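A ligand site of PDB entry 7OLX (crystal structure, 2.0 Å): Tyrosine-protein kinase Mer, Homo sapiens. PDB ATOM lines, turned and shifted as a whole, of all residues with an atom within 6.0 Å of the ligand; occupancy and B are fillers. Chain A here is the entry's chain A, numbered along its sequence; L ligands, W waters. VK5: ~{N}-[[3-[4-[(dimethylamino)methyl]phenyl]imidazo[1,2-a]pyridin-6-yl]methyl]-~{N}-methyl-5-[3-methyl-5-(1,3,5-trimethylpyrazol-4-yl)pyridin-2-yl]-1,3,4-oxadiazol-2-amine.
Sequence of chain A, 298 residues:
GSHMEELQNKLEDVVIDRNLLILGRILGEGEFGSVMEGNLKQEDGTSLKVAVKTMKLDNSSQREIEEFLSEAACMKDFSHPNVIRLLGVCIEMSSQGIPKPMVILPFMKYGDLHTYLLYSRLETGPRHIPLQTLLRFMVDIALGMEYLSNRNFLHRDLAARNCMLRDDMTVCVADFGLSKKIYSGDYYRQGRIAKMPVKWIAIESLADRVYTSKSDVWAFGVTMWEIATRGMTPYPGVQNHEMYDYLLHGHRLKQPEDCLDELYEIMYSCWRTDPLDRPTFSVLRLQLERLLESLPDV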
ATOM      1  N   LEU A  27       7.347  30.347 -35.605  1.00  0.00           N
ATOM      2  CA  LEU A  27       8.076  31.396 -34.911  1.00  0.00           C
ATOM      3  C   LEU A  27       9.582  31.117 -34.862  1.00  0.00           C
ATOM      4  O   LEU A  27      10.386  32.023 -34.996  1.00  0.00           O
ATOM      5  CB  LEU A  27       7.544  31.536 -33.481  1.00  0.00           C
ATOM      6  CG  LEU A  27       6.037  31.837 -33.381  1.00  0.00           C
ATOM      7  CD1 LEU A  27       5.518  31.624 -31.971  1.00  0.00           C
ATOM      8  CD2 LEU A  27       5.736  33.248 -33.868  1.00  0.00           C
ATOM      9  N   GLY A  28       9.943  29.859 -34.649  1.00  0.00           N
ATOM     10  CA  GLY A  28      11.333  29.404 -34.634  1.00  0.00           C
ATOM     11  C   GLY A  28      11.423  27.979 -35.124  1.00  0.00           C
ATOM     12  O   GLY A  28      10.443  27.229 -35.060  1.00  0.00           O
ATOM     13  N   GLU A  29      12.591  27.599 -35.612  1.00  0.00           N
ATOM     14  CA  GLU A  29      12.778  26.296 -36.249  1.00  0.00           C
ATOM     15  C   GLU A  29      14.259  25.967 -36.345  1.00  0.00           C
ATOM     16  O   GLU A  29      15.070  26.843 -36.657  1.00  0.00           O
ATOM     17  CB  GLU A  29      12.138  26.323 -37.643  1.00  0.00           C
ATOM     18  CG  GLU A  29      12.267  25.028 -38.434  1.00  0.00           C
ATOM     19  CD  GLU A  29      11.269  24.939 -39.574  1.00  0.00           C
ATOM     20  OE1 GLU A  29      10.799  25.999 -40.055  1.00  0.00           O
ATOM     21  OE2 GLU A  29      10.963  23.802 -39.998  1.00  0.00           O
ATOM     22  N   VAL A  35       8.944  25.762 -33.173  1.00  0.00           N
ATOM     23  CA  VAL A  35       7.979  26.457 -32.338  1.00  0.00           C
ATOM     24  C   VAL A  35       7.030  27.235 -33.238  1.00  0.00           C
ATOM     25  O   VAL A  35       7.461  27.980 -34.126  1.00  0.00           O
ATOM     26  CB  VAL A  35       8.643  27.449 -31.357  1.00  0.00           C
ATOM     27  CG1 VAL A  35       7.592  28.103 -30.462  1.00  0.00           C
ATOM     28  CG2 VAL A  35       9.703  26.731 -30.526  1.00  0.00           C
ATOM     29  N   VAL A  50      -1.666  30.006 -27.962  1.00  0.00           N
ATOM     30  CA  VAL A  50      -0.623  29.147 -27.404  1.00  0.00           C
ATOM     31  C   VAL A  50       0.620  29.115 -28.277  1.00  0.00           C
ATOM     32  O   VAL A  50       0.584  29.480 -29.441  1.00  0.00           O
ATOM     33  CB  VAL A  50      -1.134  27.701 -27.182  1.00  0.00           C
ATOM     34  CG1 VAL A  50      -2.206  27.705 -26.115  1.00  0.00           C
ATOM     35  CG2 VAL A  50      -1.669  27.075 -28.461  1.00  0.00           C
ATOM     36  N   ALA A  51       1.720  28.706 -27.657  1.00  0.00           N
ATOM     37  CA  ALA A  51       2.943  28.342 -28.358  1.00  0.00           C
ATOM     38  C   ALA A  51       2.980  26.817 -28.412  1.00  0.00           C
ATOM     39  O   ALA A  51       2.708  26.144 -27.414  1.00  0.00           O
ATOM     40  CB  ALA A  51       4.164  28.887 -27.645  1.00  0.00           C
ATOM     41  N   LYS A  53       5.418  23.648 -29.399  1.00  0.00           N
ATOM     42  CA  LYS A  53       6.763  23.167 -29.685  1.00  0.00           C
ATOM     43  C   LYS A  53       6.744  21.707 -30.129  1.00  0.00           C
ATOM     44  O   LYS A  53       6.360  20.833 -29.353  1.00  0.00           O
ATOM     45  CB  LYS A  53       7.641  23.318 -28.448  1.00  0.00           C
ATOM     46  CG  LYS A  53       9.120  23.001 -28.675  1.00  0.00           C
ATOM     47  CD  LYS A  53       9.834  23.063 -27.348  1.00  0.00           C
ATOM     48  CE  LYS A  53      11.332  23.034 -27.492  1.00  0.00           C
ATOM     49  NZ  LYS A  53      11.930  23.192 -26.132  1.00  0.00           N
ATOM     50  N   MET A  55       8.914  18.371 -31.302  1.00  0.00           N
ATOM     51  CA  MET A  55      10.236  17.812 -30.954  1.00  0.00           C
ATOM     52  C   MET A  55      10.482  16.487 -31.687  1.00  0.00           C
ATOM     53  O   MET A  55       9.553  15.718 -31.899  1.00  0.00           O
ATOM     54  CB  MET A  55      10.304  17.583 -29.442  1.00  0.00           C
ATOM     55  CG  MET A  55      10.304  18.870 -28.632  1.00  0.00           C
ATOM     56  SD  MET A  55       9.879  18.665 -26.897  1.00  0.00           S
ATOM     57  CE  MET A  55      11.266  17.701 -26.311  1.00  0.00           C
ATOM     58  N   GLU A  67       8.401   7.648 -22.171  1.00  0.00           N
ATOM     59  CA  GLU A  67       9.265   8.495 -21.327  1.00  0.00           C
ATOM     60  C   GLU A  67       8.886   9.965 -21.406  1.00  0.00           C
ATOM     61  O   GLU A  67       8.817  10.668 -20.389  1.00  0.00           O
ATOM     62  CB  GLU A  67      10.738   8.361 -21.748  1.00  0.00           C
ATOM     63  CG  GLU A  67      11.390   7.012 -21.438  1.00  0.00           C
ATOM     64  CD  GLU A  67      12.782   6.882 -22.031  1.00  0.00           C
ATOM     65  OE1 GLU A  67      13.076   5.812 -22.614  1.00  0.00           O
ATOM     66  OE2 GLU A  67      13.590   7.831 -21.904  1.00  0.00           O
ATOM     67  N   PHE A  68       8.655  10.432 -22.628  1.00  0.00           N
ATOM     68  CA  PHE A  68       8.212  11.796 -22.905  1.00  0.00           C
ATOM     69  C   PHE A  68       6.884  12.117 -22.209  1.00  0.00           C
ATOM     70  O   PHE A  68       6.756  13.138 -21.545  1.00  0.00           O
ATOM     71  CB  PHE A  68       8.105  12.003 -24.429  1.00  0.00           C
ATOM     72  CG  PHE A  68       7.603  13.364 -24.819  1.00  0.00           C
ATOM     73  CD1 PHE A  68       8.474  14.445 -24.905  1.00  0.00           C
ATOM     74  CD2 PHE A  68       6.258  13.566 -25.099  1.00  0.00           C
ATOM     75  CE1 PHE A  68       8.019  15.699 -25.257  1.00  0.00           C
ATOM     76  CE2 PHE A  68       5.792  14.823 -25.458  1.00  0.00           C
ATOM     77  CZ  PHE A  68       6.677  15.897 -25.529  1.00  0.00           C
ATOM     78  N   LEU A  69       5.892  11.235 -22.370  1.00  0.00           N
ATOM     79  CA  LEU A  69       4.574  11.429 -21.753  1.00  0.00           C
ATOM     80  C   LEU A  69       4.638  11.445 -20.231  1.00  0.00           C
ATOM     81  O   LEU A  69       3.924  12.225 -19.592  1.00  0.00           O
ATOM     82  CB  LEU A  69       3.618  10.321 -22.209  1.00  0.00           C
ATOM     83  CG  LEU A  69       3.158  10.379 -23.670  1.00  0.00           C
ATOM     84  CD1 LEU A  69       2.485   9.057 -24.033  1.00  0.00           C
ATOM     85  CD2 LEU A  69       2.230  11.559 -23.911  1.00  0.00           C
ATOM     86  N   GLU A  71       7.435  12.163 -18.339  1.00  0.00           N
ATOM     87  CA  GLU A  71       8.143  13.396 -17.995  1.00  0.00           C
ATOM     88  C   GLU A  71       7.197  14.598 -18.129  1.00  0.00           C
ATOM     89  O   GLU A  71       7.168  15.458 -17.250  1.00  0.00           O
ATOM     90  CB  GLU A  71       9.375  13.546 -18.911  1.00  0.00           C
ATOM     91  CG  GLU A  71      10.292  14.728 -18.602  1.00  0.00           C
ATOM     92  CD  GLU A  71      11.074  14.567 -17.313  1.00  0.00           C
ATOM     93  OE1 GLU A  71      11.696  13.499 -17.107  1.00  0.00           O
ATOM     94  OE2 GLU A  71      11.070  15.516 -16.488  1.00  0.00           O
ATOM     95  N   ALA A  72       6.413  14.633 -19.205  1.00  0.00           N
ATOM     96  CA  ALA A  72       5.420  15.692 -19.422  1.00  0.00           C
ATOM     97  C   ALA A  72       4.372  15.753 -18.332  1.00  0.00           C
ATOM     98  O   ALA A  72       3.936  16.839 -17.957  1.00  0.00           O
ATOM     99  CB  ALA A  72       4.752  15.525 -20.780  1.00  0.00           C
ATOM    100  N   MET A  75       5.852  17.594 -15.366  1.00  0.00           N
ATOM    101  CA  MET A  75       5.951  19.037 -15.642  1.00  0.00           C
ATOM    102  C   MET A  75       4.590  19.720 -15.653  1.00  0.00           C
ATOM    103  O   MET A  75       4.461  20.866 -15.224  1.00  0.00           O
ATOM    104  CB  MET A  75       6.639  19.288 -16.985  1.00  0.00           C
ATOM    105  CG  MET A  75       8.088  18.843 -17.039  1.00  0.00           C
ATOM    106  SD  MET A  75       8.660  18.851 -18.739  1.00  0.00           S
ATOM    107  CE  MET A  75      10.364  18.291 -18.573  1.00  0.00           C
ATOM    108  N   ILE A  84       6.932  28.115 -15.923  1.00  0.00           N
ATOM    109  CA  ILE A  84       5.996  28.037 -17.050  1.00  0.00           C
ATOM    110  C   ILE A  84       5.014  26.882 -16.845  1.00  0.00           C
ATOM    111  O   ILE A  84       5.420  25.815 -16.386  1.00  0.00           O
ATOM    112  CB  ILE A  84       6.735  27.903 -18.406  1.00  0.00           C
ATOM    113  CG1 ILE A  84       5.794  28.244 -19.574  1.00  0.00           C
ATOM    114  CG2 ILE A  84       7.353  26.517 -18.589  1.00  0.00           C
ATOM    115  CD1 ILE A  84       6.519  28.501 -20.878  1.00  0.00           C
ATOM    116  N   LEU A  86       2.911  24.018 -18.289  1.00  0.00           N
ATOM    117  CA  LEU A  86       2.688  23.164 -19.443  1.00  0.00           C
ATOM    118  C   LEU A  86       1.182  22.899 -19.560  1.00  0.00           C
ATOM    119  O   LEU A  86       0.606  22.362 -18.621  1.00  0.00           O
ATOM    120  CB  LEU A  86       3.430  21.845 -19.234  1.00  0.00           C
ATOM    121  CG  LEU A  86       3.283  20.747 -20.278  1.00  0.00           C
ATOM    122  CD1 LEU A  86       3.873  21.225 -21.574  1.00  0.00           C
ATOM    123  CD2 LEU A  86       3.982  19.494 -19.817  1.00  0.00           C
ATOM    124  N   VAL A  89       0.132  17.999 -23.919  1.00  0.00           N
ATOM    125  CA  VAL A  89       0.898  17.489 -25.056  1.00  0.00           C
ATOM    126  C   VAL A  89      -0.025  16.837 -26.085  1.00  0.00           C
ATOM    127  O   VAL A  89      -1.087  16.327 -25.741  1.00  0.00           O
ATOM    128  CB  VAL A  89       2.000  16.490 -24.608  1.00  0.00           C
ATOM    129  CG1 VAL A  89       3.038  17.201 -23.752  1.00  0.00           C
ATOM    130  CG2 VAL A  89       1.419  15.315 -23.817  1.00  0.00           C
ATOM    131  N   VAL A 103       4.395  20.026 -27.643  1.00  0.00           N
ATOM    132  CA  VAL A 103       4.210  20.584 -26.312  1.00  0.00           C
ATOM    133  C   VAL A 103       3.439  21.896 -26.448  1.00  0.00           C
ATOM    134  O   VAL A 103       3.834  22.776 -27.213  1.00  0.00           O
ATOM    135  CB  VAL A 103       5.585  20.826 -25.643  1.00  0.00           C
ATOM    136  CG1 VAL A 103       5.451  21.581 -24.329  1.00  0.00           C
ATOM    137  CG2 VAL A 103       6.313  19.514 -25.449  1.00  0.00           C
ATOM    138  N   LEU A 105       2.038  25.356 -24.782  1.00  0.00           N
ATOM    139  CA  LEU A 105       2.449  26.308 -23.754  1.00  0.00           C
ATOM    140  C   LEU A 105       1.660  27.607 -23.892  1.00  0.00           C
ATOM    141  O   LEU A 105       1.214  27.953 -24.992  1.00  0.00           O
ATOM    142  CB  LEU A 105       3.940  26.601 -23.884  1.00  0.00           C
ATOM    143  CG  LEU A 105       4.871  25.375 -23.919  1.00  0.00           C
ATOM    144  CD1 LEU A 105       6.118  25.629 -24.752  1.00  0.00           C
ATOM    145  CD2 LEU A 105       5.232  24.935 -22.510  1.00  0.00           C
ATOM    146  N   PRO A 106       1.491  28.366 -22.786  1.00  0.00           N
ATOM    147  CA  PRO A 106       0.911  29.709 -22.922  1.00  0.00           C
ATOM    148  C   PRO A 106       1.795  30.575 -23.799  1.00  0.00           C
ATOM    149  O   PRO A 106       3.015  30.447 -23.748  1.00  0.00           O
ATOM    150  CB  PRO A 106       0.888  30.263 -21.486  1.00  0.00           C
ATOM    151  CG  PRO A 106       1.256  29.121 -20.594  1.00  0.00           C
ATOM    152  CD  PRO A 106       1.939  28.081 -21.414  1.00  0.00           C
ATOM    153  N   PHE A 107       1.179  31.404 -24.623  1.00  0.00           N
ATOM    154  CA  PHE A 107       1.915  32.275 -25.517  1.00  0.00           C
ATOM    155  C   PHE A 107       2.427  33.471 -24.714  1.00  0.00           C
ATOM    156  O   PHE A 107       1.650  34.109 -23.992  1.00  0.00           O
ATOM    157  CB  PHE A 107       1.034  32.763 -26.649  1.00  0.00           C
ATOM    158  CG  PHE A 107       1.795  33.443 -27.737  1.00  0.00           C
ATOM    159  CD1 PHE A 107       2.368  32.694 -28.761  1.00  0.00           C
ATOM    160  CD2 PHE A 107       1.941  34.819 -27.749  1.00  0.00           C
ATOM    161  CE1 PHE A 107       3.073  33.312 -29.763  1.00  0.00           C
ATOM    162  CE2 PHE A 107       2.655  35.447 -28.748  1.00  0.00           C
ATOM    163  CZ  PHE A 107       3.221  34.691 -29.761  1.00  0.00           C
ATOM    164  N   MET A 108       3.729  33.756 -24.867  1.00  0.00           N
ATOM    165  CA  MET A 108       4.407  34.855 -24.169  1.00  0.00           C
ATOM    166  C   MET A 108       4.872  35.879 -25.213  1.00  0.00           C
ATOM    167  O   MET A 108       5.979  35.745 -25.791  1.00  0.00           O
ATOM    168  CB  MET A 108       5.631  34.297 -23.415  1.00  0.00           C
ATOM    169  CG  MET A 108       5.389  33.048 -22.590  1.00  0.00           C
ATOM    170  SD  MET A 108       5.019  33.437 -20.892  1.00  0.00           S
ATOM    171  CE  MET A 108       4.947  31.799 -20.180  1.00  0.00           C
ATOM    172  N   LYS A 109       4.047  36.902 -25.458  1.00  0.00           N
ATOM    173  CA  LYS A 109       4.333  37.866 -26.531  1.00  0.00           C
ATOM    174  C   LYS A 109       5.640  38.638 -26.336  1.00  0.00           C
ATOM    175  O   LYS A 109       6.296  38.950 -27.307  1.00  0.00           O
ATOM    176  CB  LYS A 109       3.143  38.808 -26.824  1.00  0.00           C
ATOM    177  CG  LYS A 109       2.741  39.760 -25.720  1.00  0.00           C
ATOM    178  CD  LYS A 109       1.570  40.628 -26.170  1.00  0.00           C
ATOM    179  CE  LYS A 109       0.934  41.385 -25.023  1.00  0.00           C
ATOM    180  NZ  LYS A 109       1.908  42.251 -24.302  1.00  0.00           N
ATOM    181  N   GLY A 111       8.329  37.345 -25.131  1.00  0.00           N
ATOM    182  CA  GLY A 111       9.405  36.424 -25.499  1.00  0.00           C
ATOM    183  C   GLY A 111      10.313  36.090 -24.330  1.00  0.00           C
ATOM    184  O   GLY A 111       9.925  36.223 -23.160  1.00  0.00           O
ATOM    185  N   ASP A 112      11.522  35.640 -24.658  1.00  0.00           N
ATOM    186  CA  ASP A 112      12.483  35.216 -23.652  1.00  0.00           C
ATOM    187  C   ASP A 112      13.226  36.408 -23.074  1.00  0.00           C
ATOM    188  O   ASP A 112      13.334  37.448 -23.704  1.00  0.00           O
ATOM    189  CB  ASP A 112      13.464  34.192 -24.208  1.00  0.00           C
ATOM    190  CG  ASP A 112      14.479  34.803 -25.157  1.00  0.00           C
ATOM    191  OD1 ASP A 112      14.137  35.029 -26.333  1.00  0.00           O
ATOM    192  OD2 ASP A 112      15.605  35.065 -24.723  1.00  0.00           O
ATOM    193  N   THR A 115      16.685  37.854 -25.050  1.00  0.00           N
ATOM    194  CA  THR A 115      16.380  38.723 -26.188  1.00  0.00           C
ATOM    195  C   THR A 115      15.832  40.077 -25.740  1.00  0.00           C
ATOM    196  O   THR A 115      16.212  41.120 -26.280  1.00  0.00           O
ATOM    197  CB  THR A 115      15.337  38.077 -27.125  1.00  0.00           C
ATOM    198  OG1 THR A 115      15.777  36.769 -27.487  1.00  0.00           O
ATOM    199  CG2 THR A 115      15.164  38.903 -28.389  1.00  0.00           C
ATOM    200  N   MET A 164      11.127  33.119 -19.462  1.00  0.00           N
ATOM    201  CA  MET A 164      10.120  33.775 -20.293  1.00  0.00           C
ATOM    202  C   MET A 164       9.457  34.920 -19.540  1.00  0.00           C
ATOM    203  O   MET A 164       9.267  34.853 -18.339  1.00  0.00           O
ATOM    204  CB  MET A 164       9.059  32.766 -20.764  1.00  0.00           C
ATOM    205  CG  MET A 164       9.617  31.645 -21.626  1.00  0.00           C
ATOM    206  SD  MET A 164      10.356  32.127 -23.200  1.00  0.00           S
ATOM    207  CE  MET A 164       8.996  32.944 -24.041  1.00  0.00           C
ATOM    208  N   ALA A 174      11.572  28.208 -17.754  1.00  0.00           N
ATOM    209  CA  ALA A 174      10.964  27.434 -18.836  1.00  0.00           C
ATOM    210  C   ALA A 174      11.993  26.546 -19.509  1.00  0.00           C
ATOM    211  O   ALA A 174      13.148  26.514 -19.116  1.00  0.00           O
ATOM    212  CB  ALA A 174      10.334  28.384 -19.847  1.00  0.00           C
ATOM    213  N   ASP A 175      11.540  25.822 -20.525  1.00  0.00           N
ATOM    214  CA  ASP A 175      12.415  25.164 -21.490  1.00  0.00           C
ATOM    215  C   ASP A 175      13.409  24.255 -20.784  1.00  0.00           C
ATOM    216  O   ASP A 175      14.619  24.303 -21.021  1.00  0.00           O
ATOM    217  CB  ASP A 175      13.114  26.246 -22.360  1.00  0.00           C
ATOM    218  CG  ASP A 175      13.063  25.935 -23.838  1.00  0.00           C
ATOM    219  OD1 ASP A 175      13.014  24.748 -24.205  1.00  0.00           O
ATOM    220  OD2 ASP A 175      13.096  26.889 -24.643  1.00  0.00           O
ATOM    221  N   PHE A 176      12.860  23.394 -19.935  1.00  0.00           N
ATOM    222  CA  PHE A 176      13.647  22.523 -19.063  1.00  0.00           C
ATOM    223  C   PHE A 176      14.564  21.609 -19.881  1.00  0.00           C
ATOM    224  O   PHE A 176      14.175  21.108 -20.940  1.00  0.00           O
ATOM    225  CB  PHE A 176      12.729  21.673 -18.180  1.00  0.00           C
ATOM    226  CG  PHE A 176      11.649  22.460 -17.498  1.00  0.00           C
ATOM    227  CD1 PHE A 176      11.973  23.469 -16.615  1.00  0.00           C
ATOM    228  CD2 PHE A 176      10.302  22.230 -17.800  1.00  0.00           C
ATOM    229  CE1 PHE A 176      10.982  24.220 -15.997  1.00  0.00           C
ATOM    230  CE2 PHE A 176       9.300  22.980 -17.181  1.00  0.00           C
ATOM    231  CZ  PHE A 176       9.648  23.983 -16.284  1.00  0.00           C
ATOM    232  N   GLY A 177      15.793  21.433 -19.395  1.00  0.00           N
ATOM    233  CA  GLY A 177      16.773  20.586 -20.069  1.00  0.00           C
ATOM    234  C   GLY A 177      16.515  19.126 -19.771  1.00  0.00           C
ATOM    235  O   GLY A 177      15.690  18.504 -20.432  1.00  0.00           O
HETATM  236  C1  VK5 L   1      13.397  34.321 -30.856  1.00  0.00           C
HETATM  237  C2  VK5 L   1      11.314  33.447 -31.738  1.00  0.00           C
HETATM  238  C3  VK5 L   1      10.282  33.130 -30.683  1.00  0.00           C
HETATM  239  N6  VK5 L   1      10.454  17.088 -22.344  1.00  0.00           N
HETATM  240  C7  VK5 L   1       8.816  33.821 -28.890  1.00  0.00           C
HETATM  241  C8  VK5 L   1       9.764  34.123 -29.850  1.00  0.00           C
HETATM  242  C9  VK5 L   1       7.326  32.177 -27.716  1.00  0.00           C
HETATM  243  C10 VK5 L   1       6.058  32.653 -27.533  1.00  0.00           C
HETATM  244  C11 VK5 L   1       6.337  31.219 -25.959  1.00  0.00           C
HETATM  245  C12 VK5 L   1       6.269  30.335 -24.846  1.00  0.00           C
HETATM  246  C13 VK5 L   1       7.343  29.572 -24.547  1.00  0.00           C
HETATM  247  C14 VK5 L   1       8.557  29.614 -25.329  1.00  0.00           C
HETATM  248  C15 VK5 L   1       9.778  28.778 -25.037  1.00  0.00           C
HETATM  249  C16 VK5 L   1       9.330  26.850 -26.547  1.00  0.00           C
HETATM  250  C19 VK5 L   1       9.281  23.319 -22.804  1.00  0.00           C
HETATM  251  C20 VK5 L   1       9.894  21.242 -23.634  1.00  0.00           C
HETATM  252  C21 VK5 L   1       9.391  20.577 -22.525  1.00  0.00           C
HETATM  253  C22 VK5 L   1       8.813  21.344 -21.514  1.00  0.00           C
HETATM  254  C24 VK5 L   1       8.098  23.510 -20.509  1.00  0.00           C
HETATM  255  C27 VK5 L   1      12.057  18.873 -22.798  1.00  0.00           C
HETATM  256  C30 VK5 L   1       7.033  18.326 -21.878  1.00  0.00           C
HETATM  257  C31 VK5 L   1       8.600  30.464 -26.384  1.00  0.00           C
HETATM  258  C29 VK5 L   1       8.500  18.162 -22.116  1.00  0.00           C
HETATM  259  N7  VK5 L   1       9.134  16.979 -22.098  1.00  0.00           N
HETATM  260  C28 VK5 L   1       8.570  15.660 -21.867  1.00  0.00           C
HETATM  261  C26 VK5 L   1      10.674  18.373 -22.514  1.00  0.00           C
HETATM  262  C25 VK5 L   1       9.462  19.106 -22.377  1.00  0.00           C
HETATM  263  N5  VK5 L   1       9.838  22.579 -23.785  1.00  0.00           N
HETATM  264  C23 VK5 L   1       8.735  22.725 -21.625  1.00  0.00           C
HETATM  265  C18 VK5 L   1       9.260  24.774 -23.043  1.00  0.00           C
HETATM  266  O   VK5 L   1       9.377  25.254 -24.327  1.00  0.00           O
HETATM  267  N3  VK5 L   1       9.154  25.706 -22.165  1.00  0.00           N
HETATM  268  N4  VK5 L   1       9.187  26.913 -22.865  1.00  0.00           N
HETATM  269  C17 VK5 L   1       9.319  26.593 -24.120  1.00  0.00           C
HETATM  270  N2  VK5 L   1       9.402  27.378 -25.195  1.00  0.00           N
HETATM  271  N8  VK5 L   1       7.520  31.245 -26.695  1.00  0.00           N
HETATM  272  N1  VK5 L   1       5.440  32.072 -26.455  1.00  0.00           N
HETATM  273  C6  VK5 L   1       8.350  32.518 -28.734  1.00  0.00           C
HETATM  274  C5  VK5 L   1       8.855  31.527 -29.574  1.00  0.00           C
HETATM  275  C4  VK5 L   1       9.812  31.840 -30.531  1.00  0.00           C
HETATM  276  N   VK5 L   1      12.684  33.127 -31.317  1.00  0.00           N
HETATM  277  C   VK5 L   1      13.438  32.467 -32.389  1.00  0.00           C
HETATM  278  O   HOH W   1      11.859  31.394 -26.681  1.00  0.00           O
HETATM  279  O   HOH W   2      12.774  29.744 -23.957  1.00  0.00           O
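The backbone NH of Met 108 lies within hydrogen-bond range of a nitrogen (N1) of the ligand (2.9 Å). N3 of the ligand is in hydrogen-bond range of N of Asp 175. A nitrogen (N5) of the ligand is in hydrogen-bond range of the side-chain amino group of Lys 53 (3.2 Å).
Water W2 lies within hydrogen-bond range of the side-chain carboxylate (OD2) of Asp 175 (3.0 Å) and the side-chain sulfur (SD) of Met 164 (3.5 Å).
NZ of Lys 53 lies within salt-bridge range of OD1 of Asp 175 (2.7 Å). N of Val 103 sits at hydrogen-bond distance from O of Lys 53 (2.7 Å). The backbone carbonyl oxygen (O) of Leu 105 lies within hydrogen-bond range of the backbone NH (N) of Ala 51 (2.8 Å). The backbone NH (N) of Leu 27 is in hydrogen-bond range of the backbone carbonyl oxygen (O) of Val 35 (2.8 Å). The backbone NH (N) of Val 35 sits at hydrogen-bond distance from the backbone carbonyl oxygen (O) of Gly 28 (2.8 Å).
Leu 27 touches the ligand (O to C2, 3.7 Å). Val 35 touches the ligand (CG1 to C5, 3.8 Å). Ala 51 touches the ligand (CB to C11, 3.6 Å). Met 55 touches the ligand (CE to C27, 3.8 Å). O of Phe 68 touches C28 of the ligand, 3.1 Å away. CB of Glu 71 touches C28 of the ligand, at 3.7 Å. N of Ala 72 touches C28 of the ligand, at 3.6 Å. Met 75 touches the ligand. CG2 of Ile 84 touches C24 of the ligand (3.6 Å). CD2 of Leu 86 touches C30 of the ligand, at 3.9 Å. CG2 of Val 103 touches C30 of the ligand, 3.8 Å away. CD1 of Leu 105 touches O of the ligand, at 3.3 Å. O of Pro 106 touches C12 of the ligand (3.4 Å). CA of Phe 107 touches N1 of the ligand (3.7 Å). CE of Met 164 touches C31 of the ligand (3.4 Å). CB of Ala 174 touches N4 of the ligand (3.5 Å). CE2 of Phe 176 touches C24 of the ligand, at 3.6 Å. Hydrophobic or aromatic side chains that line the ligand: Leu 27, Val 35, Ala 51, Met 55, Phe 68, Ala 72, Met 75, Ile 84, Leu 86, Val 103, Leu 105, Phe 107, Met 108, Met 164, Ala 174 and Phe 176. Within 4 Å of the ligand: Leu 27, Val 35, Ala 51, Lys 53, Met 55, Phe 68, Glu 71, Ala 72, Met 75, Ile 84, Leu 86, Val 103, Leu 105, Pro 106, Phe 107, Met 108, Met 164, Ala 174, Asp 175 and Phe 176.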
